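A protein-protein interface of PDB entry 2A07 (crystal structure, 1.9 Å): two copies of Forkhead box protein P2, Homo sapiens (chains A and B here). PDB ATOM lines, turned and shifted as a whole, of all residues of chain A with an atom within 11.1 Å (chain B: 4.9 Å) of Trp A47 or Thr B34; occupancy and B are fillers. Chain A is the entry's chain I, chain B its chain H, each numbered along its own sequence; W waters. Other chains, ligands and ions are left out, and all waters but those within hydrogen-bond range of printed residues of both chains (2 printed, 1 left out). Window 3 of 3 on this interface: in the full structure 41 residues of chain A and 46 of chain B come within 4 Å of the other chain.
Water W2 lies within hydrogen-bond range of the side-chain amide oxygen (OD1) of Asn A54 (2.6 Å) and the backbone NH (N) of Tyr B8 (3.4 Å).
Water W1 bridges O of Phe B37 (2.7 Å) and O of Phe A40 (2.8 Å).
The backbone carbonyl oxygen (O) of Lys A48 sits at hydrogen-bond distance from the guanidinium group (NH1) of Arg A52 (3.1 Å).
ND2 of Asn A54 lies within hydrogen-bond range of O of Ala A50, at 2.9 Å.
The side-chain hydroxyl of Thr B34 sits at hydrogen-bond distance from the backbone carbonyl oxygen of Tyr B30 (2.9 Å).
The backbone carbonyl oxygen (O) of Tyr A39 is in hydrogen-bond range of the guanidinium group (NH1) of Arg A42, 2.8 Å away.
O of Trp B32 lies within hydrogen-bond range of OG1 of Thr B36 (2.9 Å).
OG of Ser A56 is in hydrogen-bond range of O of Arg A52, 3.2 Å away.
Trp A47 touches just these residues of chain B: Tyr B8 (3.4 Å), Tyr B30 (3.4 Å), Phe B33 (3.5 Å), Thr B34 (3.5 Å) and Phe B37 (3.7 Å).
Thr B34 touches just one residue of chain A: Trp A47 (3.5 Å).
Of the printed residues of chain A, Tyr B30 touches Trp A47, Lys A48 and Arg A52.
No residue of chain A comes within 4 Å of Ser B31.
Printed residues of chain A within 4 Å of Thr B36: Pro A5 (3.5 Å), Phe A6 (3.6 Å) and Phe A40 (3.8 Å).
Printed residues of chain A within 4 Å of Phe B37: Phe A40, Arg A42 and Trp A47.
No residue of chain A comes within 4 Å of Ala B38.
Of the printed residues of chain B, Phe A6 touches Trp B32 (3.97 Å) and Thr B36 (3.6 Å).
Printed residues of chain B within 4 Å of Phe A40: Thr B36 and Phe B37.
Of the printed residues of chain B, Arg A42 touches Tyr B8 (3.1 Å) and Phe B37 (3.7 Å).
The nearest residue of chain A that does not touch Thr B34 is Lys A48 (4.7 Å).
Printed residues of chain A that touch a printed residue of chain B: Pro A5, Phe A6, Tyr A39, Phe A40, Arg A42, Trp A47, Lys A48, Ala A50, Val A51, Arg A52 and Asn A54.
Among the printed residues, no Asp or Glu carboxylate lies within 4 Å of a Lys or Arg side-chain nitrogen of the other chain.
1 position is printed for both chains.
The backbone NH of Tyr B8 is in hydrogen-bond range of the side-chain hydroxyl of Tyr A39, at 3.4 Å.
OH of Tyr B30 lies close to NH1 of Arg A52 (3.3 Å).
OH of Tyr B8 is in hydrogen-bond range of NE of Arg A42, 3.1 Å away.
Among the printed residues, merely in contact across the chains: Pro A5 with Trp B32, Pro A5 with Thr B36, Phe A6 with Trp B32, Phe A6 with Thr B36, Phe A40 with Thr B36, Phe A40 with Phe B37, Arg A42 with Phe B37, Trp A47 with Tyr B8, Trp A47 with Tyr B30, Trp A47 with Phe B33, Trp A47 with Thr B34, Trp A47 with Phe B37, Lys A48 with Tyr B30, Ala A50 with Tyr B8, Val A51 with Phe B33 and Asn A54 with Tyr B8.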
ATOM      1  N   PRO A   4     -14.439 -13.796 -12.504  1.00  0.00           N
ATOM      2  CA  PRO A   4     -14.147 -14.183 -11.121  1.00  0.00           C
ATOM      3  C   PRO A   4     -12.829 -13.564 -10.645  1.00  0.00           C
ATOM      4  O   PRO A   4     -11.899 -13.392 -11.429  1.00  0.00           O
ATOM      5  CB  PRO A   4     -14.066 -15.708 -11.198  1.00  0.00           C
ATOM      6  CG  PRO A   4     -14.952 -16.044 -12.363  1.00  0.00           C
ATOM      7  CD  PRO A   4     -14.572 -14.987 -13.361  1.00  0.00           C
ATOM      8  N   PRO A   5     -12.739 -13.212  -9.355  1.00  0.00           N
ATOM      9  CA  PRO A   5     -11.506 -12.617  -8.821  1.00  0.00           C
ATOM     10  C   PRO A   5     -10.302 -13.533  -9.057  1.00  0.00           C
ATOM     11  O   PRO A   5      -9.205 -13.067  -9.370  1.00  0.00           O
ATOM     12  CB  PRO A   5     -11.818 -12.454  -7.338  1.00  0.00           C
ATOM     13  CG  PRO A   5     -13.293 -12.214  -7.334  1.00  0.00           C
ATOM     14  CD  PRO A   5     -13.795 -13.237  -8.328  1.00  0.00           C
ATOM     15  N   PHE A   6     -10.521 -14.839  -8.910  1.00  0.00           N
ATOM     16  CA  PHE A   6      -9.473 -15.834  -9.112  1.00  0.00           C
ATOM     17  C   PHE A   6     -10.031 -17.088  -9.782  1.00  0.00           C
ATOM     18  O   PHE A   6     -11.223 -17.377  -9.686  1.00  0.00           O
ATOM     19  CB  PHE A   6      -8.849 -16.261  -7.770  1.00  0.00           C
ATOM     20  CG  PHE A   6      -8.246 -15.125  -6.982  1.00  0.00           C
ATOM     21  CD1 PHE A   6      -9.040 -14.342  -6.153  1.00  0.00           C
ATOM     22  CD2 PHE A   6      -6.891 -14.832  -7.087  1.00  0.00           C
ATOM     23  CE1 PHE A   6      -8.496 -13.279  -5.433  1.00  0.00           C
ATOM     24  CE2 PHE A   6      -6.333 -13.766  -6.366  1.00  0.00           C
ATOM     25  CZ  PHE A   6      -7.142 -12.991  -5.539  1.00  0.00           C
ATOM     26  N   ALA A  38      -4.910 -21.607   3.086  1.00  0.00           N
ATOM     27  CA  ALA A  38      -4.849 -21.397   4.532  1.00  0.00           C
ATOM     28  C   ALA A  38      -5.053 -19.908   4.847  1.00  0.00           C
ATOM     29  O   ALA A  38      -5.759 -19.552   5.790  1.00  0.00           O
ATOM     30  CB  ALA A  38      -3.500 -21.875   5.077  1.00  0.00           C
ATOM     31  N   TYR A  39      -4.443 -19.036   4.046  1.00  0.00           N
ATOM     32  CA  TYR A  39      -4.569 -17.597   4.260  1.00  0.00           C
ATOM     33  C   TYR A  39      -6.027 -17.152   4.194  1.00  0.00           C
ATOM     34  O   TYR A  39      -6.480 -16.344   5.005  1.00  0.00           O
ATOM     35  CB  TYR A  39      -3.761 -16.820   3.211  1.00  0.00           C
ATOM     36  CG  TYR A  39      -3.858 -15.316   3.345  1.00  0.00           C
ATOM     37  CD1 TYR A  39      -3.030 -14.611   4.230  1.00  0.00           C
ATOM     38  CD2 TYR A  39      -4.782 -14.592   2.597  1.00  0.00           C
ATOM     39  CE1 TYR A  39      -3.130 -13.217   4.355  1.00  0.00           C
ATOM     40  CE2 TYR A  39      -4.891 -13.206   2.717  1.00  0.00           C
ATOM     41  CZ  TYR A  39      -4.056 -12.526   3.602  1.00  0.00           C
ATOM     42  OH  TYR A  39      -4.167 -11.163   3.704  1.00  0.00           O
ATOM     43  N   PHE A  40      -6.768 -17.685   3.226  1.00  0.00           N
ATOM     44  CA  PHE A  40      -8.168 -17.300   3.058  1.00  0.00           C
ATOM     45  C   PHE A  40      -9.169 -17.939   4.009  1.00  0.00           C
ATOM     46  O   PHE A  40     -10.348 -17.581   4.001  1.00  0.00           O
ATOM     47  CB  PHE A  40      -8.595 -17.532   1.605  1.00  0.00           C
ATOM     48  CG  PHE A  40      -7.979 -16.555   0.651  1.00  0.00           C
ATOM     49  CD1 PHE A  40      -6.867 -16.898  -0.107  1.00  0.00           C
ATOM     50  CD2 PHE A  40      -8.479 -15.259   0.556  1.00  0.00           C
ATOM     51  CE1 PHE A  40      -6.263 -15.963  -0.949  1.00  0.00           C
ATOM     52  CE2 PHE A  40      -7.883 -14.320  -0.280  1.00  0.00           C
ATOM     53  CZ  PHE A  40      -6.772 -14.673  -1.033  1.00  0.00           C
ATOM     54  N   ARG A  41      -8.710 -18.872   4.833  1.00  0.00           N
ATOM     55  CA  ARG A  41      -9.609 -19.518   5.777  1.00  0.00           C
ATOM     56  C   ARG A  41      -9.861 -18.584   6.968  1.00  0.00           C
ATOM     57  O   ARG A  41      -9.428 -18.851   8.094  1.00  0.00           O
ATOM     58  CB  ARG A  41      -9.014 -20.846   6.245  1.00  0.00           C
ATOM     59  CG  ARG A  41      -9.977 -21.698   7.044  1.00  0.00           C
ATOM     60  CD  ARG A  41      -9.433 -23.086   7.289  1.00  0.00           C
ATOM     61  NE  ARG A  41     -10.426 -23.939   7.940  1.00  0.00           N
ATOM     62  CZ  ARG A  41     -10.207 -25.196   8.314  1.00  0.00           C
ATOM     63  NH1 ARG A  41      -9.023 -25.760   8.103  1.00  0.00           N
ATOM     64  NH2 ARG A  41     -11.175 -25.890   8.899  1.00  0.00           N
ATOM     65  N   ARG A  42     -10.556 -17.482   6.692  1.00  0.00           N
ATOM     66  CA  ARG A  42     -10.896 -16.464   7.689  1.00  0.00           C
ATOM     67  C   ARG A  42     -12.391 -16.134   7.569  1.00  0.00           C
ATOM     68  O   ARG A  42     -13.002 -16.390   6.534  1.00  0.00           O
ATOM     69  CB  ARG A  42     -10.083 -15.189   7.436  1.00  0.00           C
ATOM     70  CG  ARG A  42      -8.563 -15.315   7.595  1.00  0.00           C
ATOM     71  CD  ARG A  42      -7.867 -14.212   6.798  1.00  0.00           C
ATOM     72  NE  ARG A  42      -6.814 -13.511   7.531  1.00  0.00           N
ATOM     73  CZ  ARG A  42      -5.561 -13.934   7.660  1.00  0.00           C
ATOM     74  NH1 ARG A  42      -5.177 -15.073   7.104  1.00  0.00           N
ATOM     75  NH2 ARG A  42      -4.685 -13.209   8.345  1.00  0.00           N
ATOM     76  N   ASN A  43     -12.976 -15.556   8.616  1.00  0.00           N
ATOM     77  CA  ASN A  43     -14.397 -15.211   8.580  1.00  0.00           C
ATOM     78  C   ASN A  43     -14.623 -13.762   8.165  1.00  0.00           C
ATOM     79  O   ASN A  43     -13.681 -12.971   8.096  1.00  0.00           O
ATOM     80  CB  ASN A  43     -15.062 -15.469   9.942  1.00  0.00           C
ATOM     81  CG  ASN A  43     -14.564 -14.537  11.035  1.00  0.00           C
ATOM     82  OD1 ASN A  43     -14.505 -13.321  10.857  1.00  0.00           O
ATOM     83  ND2 ASN A  43     -14.228 -15.109  12.188  1.00  0.00           N
ATOM     84  N   ALA A  44     -15.879 -13.423   7.886  1.00  0.00           N
ATOM     85  CA  ALA A  44     -16.248 -12.072   7.475  1.00  0.00           C
ATOM     86  C   ALA A  44     -15.920 -11.051   8.553  1.00  0.00           C
ATOM     87  O   ALA A  44     -15.529  -9.927   8.252  1.00  0.00           O
ATOM     88  CB  ALA A  44     -17.734 -12.019   7.147  1.00  0.00           C
ATOM     89  N   ALA A  45     -16.082 -11.450   9.810  1.00  0.00           N
ATOM     90  CA  ALA A  45     -15.797 -10.562  10.930  1.00  0.00           C
ATOM     91  C   ALA A  45     -14.311 -10.209  10.970  1.00  0.00           C
ATOM     92  O   ALA A  45     -13.928  -9.113  11.385  1.00  0.00           O
ATOM     93  CB  ALA A  45     -16.204 -11.225  12.238  1.00  0.00           C
ATOM     94  N   THR A  46     -13.481 -11.149  10.529  1.00  0.00           N
ATOM     95  CA  THR A  46     -12.038 -10.969  10.521  1.00  0.00           C
ATOM     96  C   THR A  46     -11.591 -10.080   9.365  1.00  0.00           C
ATOM     97  O   THR A  46     -10.961  -9.045   9.578  1.00  0.00           O
ATOM     98  CB  THR A  46     -11.323 -12.318  10.412  1.00  0.00           C
ATOM     99  OG1 THR A  46     -11.708 -13.144  11.513  1.00  0.00           O
ATOM    100  CG2 THR A  46      -9.814 -12.123  10.464  1.00  0.00           C
ATOM    101  N   TRP A  47     -11.912 -10.476   8.135  1.00  0.00           N
ATOM    102  CA  TRP A  47     -11.504  -9.674   6.985  1.00  0.00           C
ATOM    103  C   TRP A  47     -12.172  -8.316   6.898  1.00  0.00           C
ATOM    104  O   TRP A  47     -11.562  -7.354   6.420  1.00  0.00           O
ATOM    105  CB  TRP A  47     -11.667 -10.452   5.665  1.00  0.00           C
ATOM    106  CG  TRP A  47     -13.055 -10.856   5.232  1.00  0.00           C
ATOM    107  CD1 TRP A  47     -13.578 -12.126   5.237  1.00  0.00           C
ATOM    108  CD2 TRP A  47     -14.058 -10.016   4.637  1.00  0.00           C
ATOM    109  NE1 TRP A  47     -14.834 -12.125   4.675  1.00  0.00           N
ATOM    110  CE2 TRP A  47     -15.154 -10.845   4.296  1.00  0.00           C
ATOM    111  CE3 TRP A  47     -14.135  -8.643   4.350  1.00  0.00           C
ATOM    112  CZ2 TRP A  47     -16.316 -10.347   3.688  1.00  0.00           C
ATOM    113  CZ3 TRP A  47     -15.291  -8.147   3.745  1.00  0.00           C
ATOM    114  CH2 TRP A  47     -16.363  -8.998   3.418  1.00  0.00           C
ATOM    115  N   LYS A  48     -13.408  -8.215   7.375  1.00  0.00           N
ATOM    116  CA  LYS A  48     -14.091  -6.928   7.347  1.00  0.00           C
ATOM    117  C   LYS A  48     -13.325  -5.940   8.229  1.00  0.00           C
ATOM    118  O   LYS A  48     -13.101  -4.786   7.855  1.00  0.00           O
ATOM    119  CB  LYS A  48     -15.526  -7.056   7.855  1.00  0.00           C
ATOM    120  CG  LYS A  48     -16.569  -7.145   6.760  1.00  0.00           C
ATOM    121  CD  LYS A  48     -17.964  -7.119   7.347  1.00  0.00           C
ATOM    122  CE  LYS A  48     -19.028  -7.029   6.272  1.00  0.00           C
ATOM    123  NZ  LYS A  48     -19.002  -8.205   5.362  1.00  0.00           N
ATOM    124  N   ASN A  49     -12.940  -6.395   9.416  1.00  0.00           N
ATOM    125  CA  ASN A  49     -12.187  -5.545  10.330  1.00  0.00           C
ATOM    126  C   ASN A  49     -10.845  -5.182   9.695  1.00  0.00           C
ATOM    127  O   ASN A  49     -10.450  -4.018   9.680  1.00  0.00           O
ATOM    128  CB  ASN A  49     -11.965  -6.267  11.663  1.00  0.00           C
ATOM    129  CG  ASN A  49     -10.795  -5.702  12.444  1.00  0.00           C
ATOM    130  OD1 ASN A  49      -9.687  -6.236  12.394  1.00  0.00           O
ATOM    131  ND2 ASN A  49     -11.032  -4.609  13.161  1.00  0.00           N
ATOM    132  N   ALA A  50     -10.160  -6.189   9.158  1.00  0.00           N
ATOM    133  CA  ALA A  50      -8.861  -5.997   8.521  1.00  0.00           C
ATOM    134  C   ALA A  50      -8.908  -5.010   7.348  1.00  0.00           C
ATOM    135  O   ALA A  50      -7.964  -4.236   7.138  1.00  0.00           O
ATOM    136  CB  ALA A  50      -8.319  -7.340   8.052  1.00  0.00           C
ATOM    137  N   VAL A  51      -9.996  -5.034   6.580  1.00  0.00           N
ATOM    138  CA  VAL A  51     -10.134  -4.127   5.436  1.00  0.00           C
ATOM    139  C   VAL A  51     -10.264  -2.673   5.861  1.00  0.00           C
ATOM    140  O   VAL A  51      -9.641  -1.788   5.270  1.00  0.00           O
ATOM    141  CB  VAL A  51     -11.352  -4.493   4.562  1.00  0.00           C
ATOM    142  CG1 VAL A  51     -11.625  -3.378   3.569  1.00  0.00           C
ATOM    143  CG2 VAL A  51     -11.076  -5.792   3.821  1.00  0.00           C
ATOM    144  N   ARG A  52     -11.089  -2.416   6.868  1.00  0.00           N
ATOM    145  CA  ARG A  52     -11.244  -1.053   7.353  1.00  0.00           C
ATOM    146  C   ARG A  52      -9.896  -0.589   7.924  1.00  0.00           C
ATOM    147  O   ARG A  52      -9.456   0.531   7.680  1.00  0.00           O
ATOM    148  CB  ARG A  52     -12.337  -0.989   8.426  1.00  0.00           C
ATOM    149  CG  ARG A  52     -13.729  -1.365   7.917  1.00  0.00           C
ATOM    150  CD  ARG A  52     -14.824  -0.824   8.829  1.00  0.00           C
ATOM    151  NE  ARG A  52     -14.659  -1.263  10.212  1.00  0.00           N
ATOM    152  CZ  ARG A  52     -14.845  -2.510  10.632  1.00  0.00           C
ATOM    153  NH1 ARG A  52     -15.210  -3.455   9.776  1.00  0.00           N
ATOM    154  NH2 ARG A  52     -14.663  -2.815  11.911  1.00  0.00           N
ATOM    155  N   HIS A  53      -9.243  -1.474   8.662  1.00  0.00           N
ATOM    156  CA  HIS A  53      -7.941  -1.194   9.266  1.00  0.00           C
ATOM    157  C   HIS A  53      -6.912  -0.763   8.216  1.00  0.00           C
ATOM    158  O   HIS A  53      -6.220   0.247   8.385  1.00  0.00           O
ATOM    159  CB  HIS A  53      -7.463  -2.448  10.007  1.00  0.00           C
ATOM    160  CG  HIS A  53      -6.089  -2.333  10.589  1.00  0.00           C
ATOM    161  ND1 HIS A  53      -4.947  -2.511   9.841  1.00  0.00           N
ATOM    162  CD2 HIS A  53      -5.677  -2.071  11.854  1.00  0.00           C
ATOM    163  CE1 HIS A  53      -3.886  -2.368  10.620  1.00  0.00           C
ATOM    164  NE2 HIS A  53      -4.303  -2.100  11.843  1.00  0.00           N
ATOM    165  N   ASN A  54      -6.819  -1.527   7.129  1.00  0.00           N
ATOM    166  CA  ASN A  54      -5.879  -1.227   6.048  1.00  0.00           C
ATOM    167  C   ASN A  54      -6.188   0.039   5.258  1.00  0.00           C
ATOM    168  O   ASN A  54      -5.270   0.713   4.789  1.00  0.00           O
ATOM    169  CB  ASN A  54      -5.795  -2.406   5.079  1.00  0.00           C
ATOM    170  CG  ASN A  54      -4.787  -3.435   5.513  1.00  0.00           C
ATOM    171  OD1 ASN A  54      -3.642  -3.434   5.051  1.00  0.00           O
ATOM    172  ND2 ASN A  54      -5.196  -4.317   6.417  1.00  0.00           N
ATOM    173  N   LEU A  55      -7.469   0.352   5.091  1.00  0.00           N
ATOM    174  CA  LEU A  55      -7.858   1.549   4.347  1.00  0.00           C
ATOM    175  C   LEU A  55      -7.497   2.828   5.107  1.00  0.00           C
ATOM    176  O   LEU A  55      -7.180   3.853   4.500  1.00  0.00           O
ATOM    177  CB  LEU A  55      -9.365   1.537   4.052  1.00  0.00           C
ATOM    178  CG  LEU A  55      -9.848   0.572   2.965  1.00  0.00           C
ATOM    179  CD1 LEU A  55     -11.366   0.618   2.869  1.00  0.00           C
ATOM    180  CD2 LEU A  55      -9.221   0.949   1.632  1.00  0.00           C
ATOM    181  N   SER A  56      -7.537   2.761   6.435  1.00  0.00           N
ATOM    182  CA  SER A  56      -7.222   3.924   7.258  1.00  0.00           C
ATOM    183  C   SER A  56      -5.787   3.951   7.773  1.00  0.00           C
ATOM    184  O   SER A  56      -5.396   4.887   8.470  1.00  0.00           O
ATOM    185  CB  SER A  56      -8.182   4.005   8.448  1.00  0.00           C
ATOM    186  OG  SER A  56      -8.009   2.902   9.320  1.00  0.00           O
ATOM    187  N   PHE A  61      -4.130   4.154  -0.067  1.00  0.00           N
ATOM    188  CA  PHE A  61      -5.581   4.057  -0.208  1.00  0.00           C
ATOM    189  C   PHE A  61      -6.202   5.399   0.171  1.00  0.00           C
ATOM    190  O   PHE A  61      -6.220   5.775   1.344  1.00  0.00           O
ATOM    191  CB  PHE A  61      -6.134   2.947   0.694  1.00  0.00           C
ATOM    192  CG  PHE A  61      -5.629   1.569   0.343  1.00  0.00           C
ATOM    193  CD1 PHE A  61      -5.170   0.706   1.338  1.00  0.00           C
ATOM    194  CD2 PHE A  61      -5.604   1.138  -0.979  1.00  0.00           C
ATOM    195  CE1 PHE A  61      -4.689  -0.566   1.015  1.00  0.00           C
ATOM    196  CE2 PHE A  61      -5.129  -0.129  -1.313  1.00  0.00           C
ATOM    197  CZ  PHE A  61      -4.668  -0.981  -0.315  1.00  0.00           C
ATOM    198  N   TYR B   8      -3.847  -7.857   2.878  1.00  0.00           N
ATOM    199  CA  TYR B   8      -5.096  -7.156   2.669  1.00  0.00           C
ATOM    200  C   TYR B   8      -4.898  -6.001   1.705  1.00  0.00           C
ATOM    201  O   TYR B   8      -5.798  -5.665   0.935  1.00  0.00           O
ATOM    202  CB  TYR B   8      -5.677  -6.666   3.998  1.00  0.00           C
ATOM    203  CG  TYR B   8      -6.404  -7.773   4.713  1.00  0.00           C
ATOM    204  CD1 TYR B   8      -5.759  -8.567   5.657  1.00  0.00           C
ATOM    205  CD2 TYR B   8      -7.720  -8.090   4.370  1.00  0.00           C
ATOM    206  CE1 TYR B   8      -6.406  -9.656   6.240  1.00  0.00           C
ATOM    207  CE2 TYR B   8      -8.372  -9.171   4.943  1.00  0.00           C
ATOM    208  CZ  TYR B   8      -7.713  -9.949   5.872  1.00  0.00           C
ATOM    209  OH  TYR B   8      -8.367 -11.026   6.424  1.00  0.00           O
ATOM    210  N   TYR B  30     -16.357  -4.690   0.117  1.00  0.00           N
ATOM    211  CA  TYR B  30     -16.881  -5.787   0.926  1.00  0.00           C
ATOM    212  C   TYR B  30     -17.440  -6.897   0.022  1.00  0.00           C
ATOM    213  O   TYR B  30     -17.216  -8.088   0.258  1.00  0.00           O
ATOM    214  CB  TYR B  30     -18.001  -5.291   1.844  1.00  0.00           C
ATOM    215  CG  TYR B  30     -17.550  -4.619   3.124  1.00  0.00           C
ATOM    216  CD1 TYR B  30     -18.486  -4.131   4.034  1.00  0.00           C
ATOM    217  CD2 TYR B  30     -16.194  -4.486   3.439  1.00  0.00           C
ATOM    218  CE1 TYR B  30     -18.094  -3.528   5.229  1.00  0.00           C
ATOM    219  CE2 TYR B  30     -15.789  -3.887   4.632  1.00  0.00           C
ATOM    220  CZ  TYR B  30     -16.745  -3.410   5.523  1.00  0.00           C
ATOM    221  OH  TYR B  30     -16.361  -2.815   6.708  1.00  0.00           O
ATOM    222  N   SER B  31     -18.190  -6.503  -1.002  1.00  0.00           N
ATOM    223  CA  SER B  31     -18.765  -7.477  -1.928  1.00  0.00           C
ATOM    224  C   SER B  31     -17.674  -8.288  -2.611  1.00  0.00           C
ATOM    225  O   SER B  31     -17.792  -9.511  -2.742  1.00  0.00           O
ATOM    226  CB  SER B  31     -19.608  -6.778  -2.998  1.00  0.00           C
ATOM    227  OG  SER B  31     -20.723  -6.140  -2.415  1.00  0.00           O
ATOM    228  N   TRP B  32     -16.619  -7.606  -3.053  1.00  0.00           N
ATOM    229  CA  TRP B  32     -15.509  -8.276  -3.721  1.00  0.00           C
ATOM    230  C   TRP B  32     -14.841  -9.270  -2.766  1.00  0.00           C
ATOM    231  O   TRP B  32     -14.539 -10.403  -3.148  1.00  0.00           O
ATOM    232  CB  TRP B  32     -14.486  -7.247  -4.222  1.00  0.00           C
ATOM    233  CG  TRP B  32     -13.417  -7.827  -5.098  1.00  0.00           C
ATOM    234  CD1 TRP B  32     -13.429  -7.921  -6.463  1.00  0.00           C
ATOM    235  CD2 TRP B  32     -12.176  -8.394  -4.669  1.00  0.00           C
ATOM    236  NE1 TRP B  32     -12.268  -8.507  -6.910  1.00  0.00           N
ATOM    237  CE2 TRP B  32     -11.481  -8.808  -5.827  1.00  0.00           C
ATOM    238  CE3 TRP B  32     -11.584  -8.593  -3.417  1.00  0.00           C
ATOM    239  CZ2 TRP B  32     -10.216  -9.409  -5.769  1.00  0.00           C
ATOM    240  CZ3 TRP B  32     -10.323  -9.192  -3.358  1.00  0.00           C
ATOM    241  CH2 TRP B  32      -9.655  -9.592  -4.531  1.00  0.00           C
ATOM    242  N   PHE B  33     -14.600  -8.859  -1.524  1.00  0.00           N
ATOM    243  CA  PHE B  33     -13.997  -9.782  -0.565  1.00  0.00           C
ATOM    244  C   PHE B  33     -14.923 -10.964  -0.275  1.00  0.00           C
ATOM    245  O   PHE B  33     -14.462 -12.095  -0.134  1.00  0.00           O
ATOM    246  CB  PHE B  33     -13.654  -9.066   0.745  1.00  0.00           C
ATOM    247  CG  PHE B  33     -12.282  -8.450   0.754  1.00  0.00           C
ATOM    248  CD1 PHE B  33     -11.256  -9.026   1.497  1.00  0.00           C
ATOM    249  CD2 PHE B  33     -12.012  -7.305   0.010  1.00  0.00           C
ATOM    250  CE1 PHE B  33      -9.977  -8.470   1.503  1.00  0.00           C
ATOM    251  CE2 PHE B  33     -10.734  -6.739   0.005  1.00  0.00           C
ATOM    252  CZ  PHE B  33      -9.715  -7.326   0.755  1.00  0.00           C
ATOM    253  N   THR B  34     -16.226 -10.706  -0.168  1.00  0.00           N
ATOM    254  CA  THR B  34     -17.179 -11.786   0.094  1.00  0.00           C
ATOM    255  C   THR B  34     -17.052 -12.839  -1.013  1.00  0.00           C
ATOM    256  O   THR B  34     -16.938 -14.034  -0.739  1.00  0.00           O
ATOM    257  CB  THR B  34     -18.636 -11.264   0.134  1.00  0.00           C
ATOM    258  OG1 THR B  34     -18.787 -10.341   1.220  1.00  0.00           O
ATOM    259  CG2 THR B  34     -19.614 -12.422   0.334  1.00  0.00           C
ATOM    260  N   ARG B  35     -17.064 -12.388  -2.262  1.00  0.00           N
ATOM    261  CA  ARG B  35     -16.923 -13.301  -3.400  1.00  0.00           C
ATOM    262  C   ARG B  35     -15.601 -14.052  -3.315  1.00  0.00           C
ATOM    263  O   ARG B  35     -15.536 -15.260  -3.523  1.00  0.00           O
ATOM    264  CB  ARG B  35     -16.930 -12.535  -4.726  1.00  0.00           C
ATOM    265  CG  ARG B  35     -18.287 -12.235  -5.328  1.00  0.00           C
ATOM    266  CD  ARG B  35     -18.093 -11.747  -6.756  1.00  0.00           C
ATOM    267  NE  ARG B  35     -19.348 -11.540  -7.473  1.00  0.00           N
ATOM    268  CZ  ARG B  35     -19.419 -11.254  -8.770  1.00  0.00           C
ATOM    269  NH1 ARG B  35     -18.307 -11.144  -9.484  1.00  0.00           N
ATOM    270  NH2 ARG B  35     -20.600 -11.078  -9.355  1.00  0.00           N
ATOM    271  N   THR B  36     -14.536 -13.323  -3.014  1.00  0.00           N
ATOM    272  CA  THR B  36     -13.214 -13.927  -2.937  1.00  0.00           C
ATOM    273  C   THR B  36     -13.077 -14.981  -1.847  1.00  0.00           C
ATOM    274  O   THR B  36     -12.614 -16.094  -2.105  1.00  0.00           O
ATOM    275  CB  THR B  36     -12.141 -12.830  -2.764  1.00  0.00           C
ATOM    276  OG1 THR B  36     -12.167 -11.976  -3.912  1.00  0.00           O
ATOM    277  CG2 THR B  36     -10.759 -13.424  -2.633  1.00  0.00           C
ATOM    278  N   PHE B  37     -13.476 -14.656  -0.626  1.00  0.00           N
ATOM    279  CA  PHE B  37     -13.357 -15.639   0.435  1.00  0.00           C
ATOM    280  C   PHE B  37     -14.287 -16.814   0.198  1.00  0.00           C
ATOM    281  O   PHE B  37     -13.972 -17.937   0.584  1.00  0.00           O
ATOM    282  CB  PHE B  37     -13.613 -15.006   1.803  1.00  0.00           C
ATOM    283  CG  PHE B  37     -12.410 -14.290   2.354  1.00  0.00           C
ATOM    284  CD1 PHE B  37     -11.945 -13.127   1.745  1.00  0.00           C
ATOM    285  CD2 PHE B  37     -11.703 -14.810   3.442  1.00  0.00           C
ATOM    286  CE1 PHE B  37     -10.788 -12.484   2.207  1.00  0.00           C
ATOM    287  CE2 PHE B  37     -10.544 -14.175   3.915  1.00  0.00           C
ATOM    288  CZ  PHE B  37     -10.087 -13.011   3.294  1.00  0.00           C
ATOM    289  N   ALA B  38     -15.419 -16.557  -0.452  1.00  0.00           N
ATOM    290  CA  ALA B  38     -16.374 -17.621  -0.750  1.00  0.00           C
ATOM    291  C   ALA B  38     -15.706 -18.625  -1.681  1.00  0.00           C
ATOM    292  O   ALA B  38     -15.828 -19.829  -1.486  1.00  0.00           O
ATOM    293  CB  ALA B  38     -17.625 -17.048  -1.411  1.00  0.00           C
HETATM  294  O   HOH W   1     -12.748 -18.445   2.925  1.00  0.00           O
HETATM  295  O   HOH W   2      -2.083  -5.334   4.371  1.00  0.00           O
